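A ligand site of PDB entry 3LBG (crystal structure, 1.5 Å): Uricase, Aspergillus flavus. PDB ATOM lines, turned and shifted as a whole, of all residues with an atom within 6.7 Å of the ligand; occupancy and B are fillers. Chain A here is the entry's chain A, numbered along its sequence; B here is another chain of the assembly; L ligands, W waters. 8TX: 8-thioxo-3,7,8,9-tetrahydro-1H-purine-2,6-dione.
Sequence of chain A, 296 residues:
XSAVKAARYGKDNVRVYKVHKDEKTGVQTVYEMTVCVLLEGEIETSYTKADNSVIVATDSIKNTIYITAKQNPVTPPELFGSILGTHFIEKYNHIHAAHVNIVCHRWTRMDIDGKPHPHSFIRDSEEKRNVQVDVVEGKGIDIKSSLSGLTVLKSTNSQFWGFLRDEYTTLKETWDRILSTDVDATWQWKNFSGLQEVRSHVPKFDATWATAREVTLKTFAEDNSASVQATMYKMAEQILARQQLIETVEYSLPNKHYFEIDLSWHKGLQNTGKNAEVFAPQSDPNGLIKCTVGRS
CZ of Phe 160 touches C5 of the ligand, at 3.4 Å. Leu 171 touches the ligand. CA of Ser 227 touches O2 of the ligand (3.3 Å). Asn 255 touches the ligand. CD1 of Ile 289 touches O6 of the ligand, at 3.8 Å. CD2 of Tyr 9 of chain B touches O6 of the ligand (3.7 Å). Ile 55 of chain B touches the ligand. Ala 57 of chain B touches the ligand (CA to N7, 3.9 Å). Hydrophobic or aromatic side chains that line the ligand: Phe 160, Leu 171, Val 228, Ile 289, Tyr 9 of chain B and Ile 55 of chain B.
Water W1 lies within hydrogen-bond range of a nitrogen (N9) of the ligand (2.8 Å) and the guanidinium group (NH1) of Arg 177 (3.2 Å). Water W2 lies within hydrogen-bond range of the side-chain hydroxyl (OG1) of Thr 58 of chain B (2.8 Å), the side-chain amide nitrogen (ND2) of Asn 255 (3.0 Å) and a nitrogen (N7) of the ligand (3.4 Å).
The backbone NH of Arg 177 is in hydrogen-bond range of the backbone carbonyl oxygen of Ser 158 (2.9 Å). OG1 of Thr 58 of chain B is in hydrogen-bond range of NZ of Lys 11 of chain B (2.9 Å). O of Ser 227 sits at hydrogen-bond distance from OG of Ser 225 (2.9 Å). OG of Ser 227 lies within hydrogen-bond range of N of Ala 230. O of Asn 255 sits at hydrogen-bond distance from NE2 of His 257, 3.3 Å away. The backbone NH (N) of Asn 255 sits at hydrogen-bond distance from the backbone carbonyl oxygen (O) of Gly 287 (2.9 Å). The side-chain hydroxyl (OH) of Tyr 9 of chain B lies within hydrogen-bond range of the backbone carbonyl oxygen (O) of Val 56 of chain B, at 2.7 Å.
The backbone NH of Val 228 lies within hydrogen-bond range of an oxygen (O2) of the ligand (2.7 Å). NH2 of Arg 177 is in hydrogen-bond range of O2 of the ligand (2.9 Å). A sulfur (S8) of the ligand lies close to the backbone NH (N) of Thr 58 of chain B (3.6 Å). The side-chain hydroxyl (OG1) of Thr 58 of chain B is in hydrogen-bond range of a nitrogen (N7) of the ligand (3.2 Å). The side-chain amide oxygen of Gln 229 sits at hydrogen-bond distance from a nitrogen (N1) of the ligand (3.0 Å). N of Asp 59 of chain B sits close to S8 of the ligand (3.2 Å).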
ATOM      1  N   SER A 158     -17.850  -9.063  16.772  1.00  0.00           N
ATOM      2  CA  SER A 158     -19.090  -9.418  17.394  1.00  0.00           C
ATOM      3  C   SER A 158     -19.693  -8.164  18.010  1.00  0.00           C
ATOM      4  O   SER A 158     -18.979  -7.350  18.598  1.00  0.00           O
ATOM      5  CB  SER A 158     -18.925 -10.531  18.431  1.00  0.00           C
ATOM      6  OG  SER A 158     -20.052 -10.778  19.231  1.00  0.00           O
ATOM      7  N   GLN A 159     -20.995  -8.019  17.857  1.00  0.00           N
ATOM      8  CA  GLN A 159     -21.717  -6.887  18.414  1.00  0.00           C
ATOM      9  C   GLN A 159     -22.980  -7.316  19.135  1.00  0.00           C
ATOM     10  O   GLN A 159     -23.493  -8.417  18.917  1.00  0.00           O
ATOM     11  CB  GLN A 159     -22.064  -5.966  17.237  1.00  0.00           C
ATOM     12  CG  GLN A 159     -20.912  -5.584  16.348  1.00  0.00           C
ATOM     13  CD  GLN A 159     -21.333  -4.572  15.275  1.00  0.00           C
ATOM     14  OE1 GLN A 159     -22.028  -3.603  15.590  1.00  0.00           O
ATOM     15  NE2 GLN A 159     -20.921  -4.854  14.061  1.00  0.00           N
ATOM     16  N   PHE A 160     -23.518  -6.468  20.009  1.00  0.00           N
ATOM     17  CA  PHE A 160     -24.823  -6.697  20.608  1.00  0.00           C
ATOM     18  C   PHE A 160     -25.415  -5.376  21.083  1.00  0.00           C
ATOM     19  O   PHE A 160     -25.129  -4.854  22.163  1.00  0.00           O
ATOM     20  CB  PHE A 160     -24.757  -7.732  21.734  1.00  0.00           C
ATOM     21  CG  PHE A 160     -26.136  -8.225  22.146  1.00  0.00           C
ATOM     22  CD1 PHE A 160     -26.938  -8.861  21.202  1.00  0.00           C
ATOM     23  CD2 PHE A 160     -26.603  -8.019  23.433  1.00  0.00           C
ATOM     24  CE1 PHE A 160     -28.198  -9.296  21.595  1.00  0.00           C
ATOM     25  CE2 PHE A 160     -27.867  -8.465  23.833  1.00  0.00           C
ATOM     26  CZ  PHE A 160     -28.662  -9.079  22.874  1.00  0.00           C
ATOM     27  N   PHE A 163     -31.132  -4.282  21.688  1.00  0.00           N
ATOM     28  CA  PHE A 163     -31.983  -5.178  22.448  1.00  0.00           C
ATOM     29  C   PHE A 163     -33.014  -4.452  23.287  1.00  0.00           C
ATOM     30  O   PHE A 163     -32.823  -3.229  23.475  1.00  0.00           O
ATOM     31  CB  PHE A 163     -31.174  -6.103  23.394  1.00  0.00           C
ATOM     32  CG  PHE A 163     -30.079  -5.370  24.175  1.00  0.00           C
ATOM     33  CD1 PHE A 163     -28.821  -5.204  23.632  1.00  0.00           C
ATOM     34  CD2 PHE A 163     -30.373  -4.895  25.439  1.00  0.00           C
ATOM     35  CE1 PHE A 163     -27.797  -4.574  24.348  1.00  0.00           C
ATOM     36  CE2 PHE A 163     -29.362  -4.234  26.130  1.00  0.00           C
ATOM     37  CZ  PHE A 163     -28.102  -4.047  25.581  1.00  0.00           C
ATOM     38  N   LEU A 171     -27.438  -3.735  31.094  1.00  0.00           N
ATOM     39  CA  LEU A 171     -26.427  -4.012  30.119  1.00  0.00           C
ATOM     40  C   LEU A 171     -26.230  -2.875  29.124  1.00  0.00           C
ATOM     41  O   LEU A 171     -27.191  -2.362  28.528  1.00  0.00           O
ATOM     42  CB  LEU A 171     -26.822  -5.288  29.317  1.00  0.00           C
ATOM     43  CG  LEU A 171     -25.787  -5.664  28.246  1.00  0.00           C
ATOM     44  CD1 LEU A 171     -24.548  -6.250  28.926  1.00  0.00           C
ATOM     45  CD2 LEU A 171     -26.304  -6.626  27.198  1.00  0.00           C
ATOM     46  N   ARG A 177     -17.284  -6.627  20.800  1.00  0.00           N
ATOM     47  CA  ARG A 177     -17.137  -7.492  21.963  1.00  0.00           C
ATOM     48  C   ARG A 177     -16.441  -8.790  21.500  1.00  0.00           C
ATOM     49  O   ARG A 177     -16.354  -9.110  20.329  1.00  0.00           O
ATOM     50  CB  ARG A 177     -18.463  -7.785  22.654  1.00  0.00           C
ATOM     51  CG  ARG A 177     -19.423  -8.681  21.856  1.00  0.00           C
ATOM     52  CD  ARG A 177     -20.724  -9.029  22.527  1.00  0.00           C
ATOM     53  NE  ARG A 177     -21.522  -9.983  21.711  1.00  0.00           N
ATOM     54  CZ  ARG A 177     -22.637 -10.539  22.191  1.00  0.00           C
ATOM     55  NH1 ARG A 177     -23.152 -10.329  23.374  1.00  0.00           N
ATOM     56  NH2 ARG A 177     -23.255 -11.384  21.339  1.00  0.00           N
ATOM     57  N   LEU A 179     -16.637 -12.799  21.457  1.00  0.00           N
ATOM     58  CA  LEU A 179     -17.599 -13.910  21.428  1.00  0.00           C
ATOM     59  C   LEU A 179     -16.869 -15.251  21.510  1.00  0.00           C
ATOM     60  O   LEU A 179     -16.018 -15.577  20.695  1.00  0.00           O
ATOM     61  CB  LEU A 179     -18.466 -13.830  20.157  1.00  0.00           C
ATOM     62  CG  LEU A 179     -19.516 -14.942  20.037  1.00  0.00           C
ATOM     63  CD1 LEU A 179     -20.511 -14.956  21.197  1.00  0.00           C
ATOM     64  CD2 LEU A 179     -20.222 -14.802  18.688  1.00  0.00           C
ATOM     65  N   SER A 225     -20.979 -10.413  13.600  1.00  0.00           N
ATOM     66  CA  SER A 225     -22.151 -10.944  14.248  1.00  0.00           C
ATOM     67  C   SER A 225     -22.990  -9.905  14.956  1.00  0.00           C
ATOM     68  O   SER A 225     -22.542  -9.146  15.820  1.00  0.00           O
ATOM     69  CB  SER A 225     -21.688 -11.998  15.289  1.00  0.00           C
ATOM     70  OG  SER A 225     -22.752 -12.421  16.103  1.00  0.00           O
ATOM     71  N   ALA A 226     -24.264  -9.868  14.616  1.00  0.00           N
ATOM     72  CA  ALA A 226     -25.257  -9.024  15.257  1.00  0.00           C
ATOM     73  C   ALA A 226     -25.738  -9.565  16.575  1.00  0.00           C
ATOM     74  O   ALA A 226     -26.287  -8.911  17.455  1.00  0.00           O
ATOM     75  CB  ALA A 226     -26.423  -8.872  14.265  1.00  0.00           C
ATOM     76  N   SER A 227     -25.578 -10.885  16.789  1.00  0.00           N
ATOM     77  CA  SER A 227     -26.009 -11.644  17.936  1.00  0.00           C
ATOM     78  C   SER A 227     -25.677 -13.124  17.676  1.00  0.00           C
ATOM     79  O   SER A 227     -25.411 -13.505  16.539  1.00  0.00           O
ATOM     80  CB  SER A 227     -27.510 -11.506  18.271  1.00  0.00           C
ATOM     81  OG  SER A 227     -28.276 -12.130  17.258  1.00  0.00           O
ATOM     82  N   VAL A 228     -25.668 -13.860  18.780  1.00  0.00           N
ATOM     83  CA  VAL A 228     -25.423 -15.316  18.660  1.00  0.00           C
ATOM     84  C   VAL A 228     -26.530 -15.939  17.779  1.00  0.00           C
ATOM     85  O   VAL A 228     -26.208 -16.755  16.902  1.00  0.00           O
ATOM     86  CB  VAL A 228     -25.382 -15.964  20.035  1.00  0.00           C
ATOM     87  CG1 VAL A 228     -25.232 -17.493  19.911  1.00  0.00           C
ATOM     88  CG2 VAL A 228     -24.204 -15.425  20.836  1.00  0.00           C
ATOM     89  N   GLN A 229     -27.760 -15.551  18.013  1.00  0.00           N
ATOM     90  CA  GLN A 229     -28.949 -16.016  17.264  1.00  0.00           C
ATOM     91  C   GLN A 229     -28.740 -15.838  15.765  1.00  0.00           C
ATOM     92  O   GLN A 229     -28.896 -16.731  14.902  1.00  0.00           O
ATOM     93  CB  GLN A 229     -30.192 -15.225  17.699  1.00  0.00           C
ATOM     94  CG  GLN A 229     -30.712 -15.384  19.099  1.00  0.00           C
ATOM     95  CD  GLN A 229     -30.115 -14.603  20.236  1.00  0.00           C
ATOM     96  OE1 GLN A 229     -29.012 -14.086  20.108  1.00  0.00           O
ATOM     97  NE2 GLN A 229     -30.764 -14.502  21.411  1.00  0.00           N
ATOM     98  N   ALA A 230     -28.350 -14.650  15.298  1.00  0.00           N
ATOM     99  CA  ALA A 230     -28.243 -14.361  13.868  1.00  0.00           C
ATOM    100  C   ALA A 230     -27.118 -15.115  13.220  1.00  0.00           C
ATOM    101  O   ALA A 230     -27.168 -15.600  12.097  1.00  0.00           O
ATOM    102  CB  ALA A 230     -28.070 -12.839  13.701  1.00  0.00           C
ATOM    103  N   ASN A 255     -23.116 -18.469  25.442  1.00  0.00           N
ATOM    104  CA  ASN A 255     -22.349 -17.232  25.371  1.00  0.00           C
ATOM    105  C   ASN A 255     -21.450 -17.143  26.620  1.00  0.00           C
ATOM    106  O   ASN A 255     -21.912 -16.833  27.689  1.00  0.00           O
ATOM    107  CB  ASN A 255     -23.310 -16.053  25.279  1.00  0.00           C
ATOM    108  CG  ASN A 255     -22.597 -14.788  24.877  1.00  0.00           C
ATOM    109  OD1 ASN A 255     -21.412 -14.759  24.579  1.00  0.00           O
ATOM    110  ND2 ASN A 255     -23.370 -13.710  24.829  1.00  0.00           N
ATOM    111  N   HIS A 257     -19.022 -15.553  28.657  1.00  0.00           N
ATOM    112  CA  HIS A 257     -18.749 -14.113  28.720  1.00  0.00           C
ATOM    113  C   HIS A 257     -17.310 -13.769  29.120  1.00  0.00           C
ATOM    114  O   HIS A 257     -16.766 -14.449  29.996  1.00  0.00           O
ATOM    115  CB  HIS A 257     -19.716 -13.445  29.706  1.00  0.00           C
ATOM    116  CG  HIS A 257     -21.170 -13.733  29.433  1.00  0.00           C
ATOM    117  ND1 HIS A 257     -21.817 -13.254  28.310  1.00  0.00           N
ATOM    118  CD2 HIS A 257     -22.087 -14.400  30.154  1.00  0.00           C
ATOM    119  CE1 HIS A 257     -23.069 -13.661  28.359  1.00  0.00           C
ATOM    120  NE2 HIS A 257     -23.286 -14.355  29.456  1.00  0.00           N
ATOM    121  N   GLY A 287     -25.072 -16.903  28.924  1.00  0.00           N
ATOM    122  CA  GLY A 287     -26.247 -16.975  28.024  1.00  0.00           C
ATOM    123  C   GLY A 287     -26.288 -18.363  27.384  1.00  0.00           C
ATOM    124  O   GLY A 287     -25.276 -19.062  27.222  1.00  0.00           O
ATOM    125  N   ILE A 289     -28.316 -20.011  23.928  1.00  0.00           N
ATOM    126  CA  ILE A 289     -29.123 -19.640  22.760  1.00  0.00           C
ATOM    127  C   ILE A 289     -29.360 -20.882  21.931  1.00  0.00           C
ATOM    128  O   ILE A 289     -28.404 -21.565  21.550  1.00  0.00           O
ATOM    129  CB  ILE A 289     -28.383 -18.553  21.966  1.00  0.00           C
ATOM    130  CG1 ILE A 289     -27.750 -17.447  22.860  1.00  0.00           C
ATOM    131  CG2 ILE A 289     -29.228 -17.941  20.878  1.00  0.00           C
ATOM    132  CD1 ILE A 289     -28.756 -16.585  23.588  1.00  0.00           C
ATOM    133  N   TYR B   9     -34.117 -19.080  24.245  1.00  0.00           N
ATOM    134  CA  TYR B   9     -32.845 -18.462  24.619  1.00  0.00           C
ATOM    135  C   TYR B   9     -33.036 -17.981  26.050  1.00  0.00           C
ATOM    136  O   TYR B   9     -34.114 -17.767  26.582  1.00  0.00           O
ATOM    137  CB  TYR B   9     -32.427 -17.355  23.617  1.00  0.00           C
ATOM    138  CG  TYR B   9     -33.096 -16.094  24.076  1.00  0.00           C
ATOM    139  CD1 TYR B   9     -34.470 -15.947  23.910  1.00  0.00           C
ATOM    140  CD2 TYR B   9     -32.350 -15.087  24.704  1.00  0.00           C
ATOM    141  CE1 TYR B   9     -35.127 -14.800  24.320  1.00  0.00           C
ATOM    142  CE2 TYR B   9     -33.035 -13.966  25.130  1.00  0.00           C
ATOM    143  CZ  TYR B   9     -34.394 -13.824  24.936  1.00  0.00           C
ATOM    144  OH  TYR B   9     -35.006 -12.687  25.391  1.00  0.00           O
ATOM    145  N   GLY B  10     -31.874 -17.736  26.734  1.00  0.00           N
ATOM    146  CA  GLY B  10     -31.988 -17.248  28.104  1.00  0.00           C
ATOM    147  C   GLY B  10     -30.643 -17.338  28.834  1.00  0.00           C
ATOM    148  O   GLY B  10     -29.604 -17.271  28.185  1.00  0.00           O
ATOM    149  N   LYS B  11     -30.761 -17.495  30.157  1.00  0.00           N
ATOM    150  CA  LYS B  11     -29.562 -17.526  31.005  1.00  0.00           C
ATOM    151  C   LYS B  11     -29.522 -18.850  31.771  1.00  0.00           C
ATOM    152  O   LYS B  11     -30.490 -19.212  32.416  1.00  0.00           O
ATOM    153  CB  LYS B  11     -29.532 -16.314  31.950  1.00  0.00           C
ATOM    154  CG  LYS B  11     -28.138 -16.070  32.559  1.00  0.00           C
ATOM    155  CD  LYS B  11     -27.125 -15.546  31.590  1.00  0.00           C
ATOM    156  CE  LYS B  11     -26.585 -14.157  31.906  1.00  0.00           C
ATOM    157  NZ  LYS B  11     -25.862 -13.592  30.750  1.00  0.00           N
ATOM    158  N   ASN B  52     -32.763  -7.338  17.085  1.00  0.00           N
ATOM    159  CA  ASN B  52     -32.590  -7.558  18.511  1.00  0.00           C
ATOM    160  C   ASN B  52     -33.671  -6.936  19.397  1.00  0.00           C
ATOM    161  O   ASN B  52     -33.686  -7.139  20.616  1.00  0.00           O
ATOM    162  CB  ASN B  52     -31.197  -7.042  18.952  1.00  0.00           C
ATOM    163  CG  ASN B  52     -30.065  -7.913  18.458  1.00  0.00           C
ATOM    164  OD1 ASN B  52     -30.287  -9.118  18.155  1.00  0.00           O
ATOM    165  ND2 ASN B  52     -28.851  -7.412  18.338  1.00  0.00           N
ATOM    166  N   ILE B  55     -35.375  -9.258  21.709  1.00  0.00           N
ATOM    167  CA  ILE B  55     -34.595  -9.915  22.756  1.00  0.00           C
ATOM    168  C   ILE B  55     -34.574  -9.172  24.091  1.00  0.00           C
ATOM    169  O   ILE B  55     -34.123  -8.020  24.139  1.00  0.00           O
ATOM    170  CB  ILE B  55     -33.143 -10.136  22.290  1.00  0.00           C
ATOM    171  CG1 ILE B  55     -32.989 -10.942  20.999  1.00  0.00           C
ATOM    172  CG2 ILE B  55     -32.332 -10.767  23.425  1.00  0.00           C
ATOM    173  CD1 ILE B  55     -31.535 -11.087  20.582  1.00  0.00           C
ATOM    174  N   VAL B  56     -35.055  -9.873  25.109  1.00  0.00           N
ATOM    175  CA  VAL B  56     -34.869  -9.541  26.514  1.00  0.00           C
ATOM    176  C   VAL B  56     -33.455 -10.052  26.808  1.00  0.00           C
ATOM    177  O   VAL B  56     -33.248 -11.271  26.791  1.00  0.00           O
ATOM    178  CB  VAL B  56     -35.901 -10.184  27.430  1.00  0.00           C
ATOM    179  CG1 VAL B  56     -35.645  -9.880  28.900  1.00  0.00           C
ATOM    180  CG2 VAL B  56     -37.301  -9.728  27.009  1.00  0.00           C
ATOM    181  N   ALA B  57     -32.509  -9.157  27.030  1.00  0.00           N
ATOM    182  CA  ALA B  57     -31.106  -9.574  27.095  1.00  0.00           C
ATOM    183  C   ALA B  57     -30.925 -10.593  28.215  1.00  0.00           C
ATOM    184  O   ALA B  57     -31.601 -10.529  29.233  1.00  0.00           O
ATOM    185  CB  ALA B  57     -30.209  -8.372  27.323  1.00  0.00           C
ATOM    186  N   THR B  58     -29.973 -11.534  27.969  1.00  0.00           N
ATOM    187  CA  THR B  58     -29.835 -12.590  29.003  1.00  0.00           C
ATOM    188  C   THR B  58     -29.366 -12.030  30.331  1.00  0.00           C
ATOM    189  O   THR B  58     -29.737 -12.548  31.392  1.00  0.00           O
ATOM    190  CB  THR B  58     -28.923 -13.749  28.561  1.00  0.00           C
ATOM    191  OG1 THR B  58     -27.559 -13.383  28.369  1.00  0.00           O
ATOM    192  CG2 THR B  58     -29.356 -14.333  27.213  1.00  0.00           C
ATOM    193  N   ASP B  59     -28.597 -10.927  30.191  1.00  0.00           N
ATOM    194  CA  ASP B  59     -28.218 -10.248  31.437  1.00  0.00           C
ATOM    195  C   ASP B  59     -29.402  -9.688  32.203  1.00  0.00           C
ATOM    196  O   ASP B  59     -29.455  -9.634  33.436  1.00  0.00           O
ATOM    197  CB  ASP B  59     -27.261  -9.098  31.084  1.00  0.00           C
ATOM    198  CG  ASP B  59     -26.684  -8.452  32.323  1.00  0.00           C
ATOM    199  OD1 ASP B  59     -25.743  -9.019  32.922  1.00  0.00           O
ATOM    200  OD2 ASP B  59     -27.150  -7.348  32.700  1.00  0.00           O
ATOM    201  N   SER B  60     -30.410  -9.233  31.425  1.00  0.00           N
ATOM    202  CA  SER B  60     -31.618  -8.780  32.125  1.00  0.00           C
ATOM    203  C   SER B  60     -32.448  -9.881  32.746  1.00  0.00           C
ATOM    204  O   SER B  60     -33.080  -9.739  33.755  1.00  0.00           O
ATOM    205  CB  SER B  60     -32.553  -7.991  31.159  1.00  0.00           C
ATOM    206  OG  SER B  60     -31.755  -7.020  30.488  1.00  0.00           O
HETATM  207  N1  8TX L   1     -27.717 -12.743  22.464  1.00  0.00           N
HETATM  208  C2  8TX L   1     -26.450 -12.348  22.170  1.00  0.00           C
HETATM  209  O2  8TX L   1     -25.913 -12.510  21.132  1.00  0.00           O
HETATM  210  N3  8TX L   1     -25.700 -11.702  23.146  1.00  0.00           N
HETATM  211  C4  8TX L   1     -26.301 -11.480  24.299  1.00  0.00           C
HETATM  212  C5  8TX L   1     -27.612 -11.821  24.602  1.00  0.00           C
HETATM  213  C6  8TX L   1     -28.422 -12.496  23.636  1.00  0.00           C
HETATM  214  O6  8TX L   1     -29.568 -12.859  23.780  1.00  0.00           O
HETATM  215  N7  8TX L   1     -27.958 -11.430  25.824  1.00  0.00           N
HETATM  216  C8  8TX L   1     -26.821 -10.834  26.330  1.00  0.00           C
HETATM  217  S8  8TX L   1     -26.641 -10.225  27.791  1.00  0.00           S
HETATM  218  N9  8TX L   1     -25.810 -10.842  25.402  1.00  0.00           N
HETATM  219  O   HOH W   1     -23.417  -9.918  26.507  1.00  0.00           O
HETATM  220  O   HOH W   2     -26.078 -14.232  26.113  1.00  0.00           O
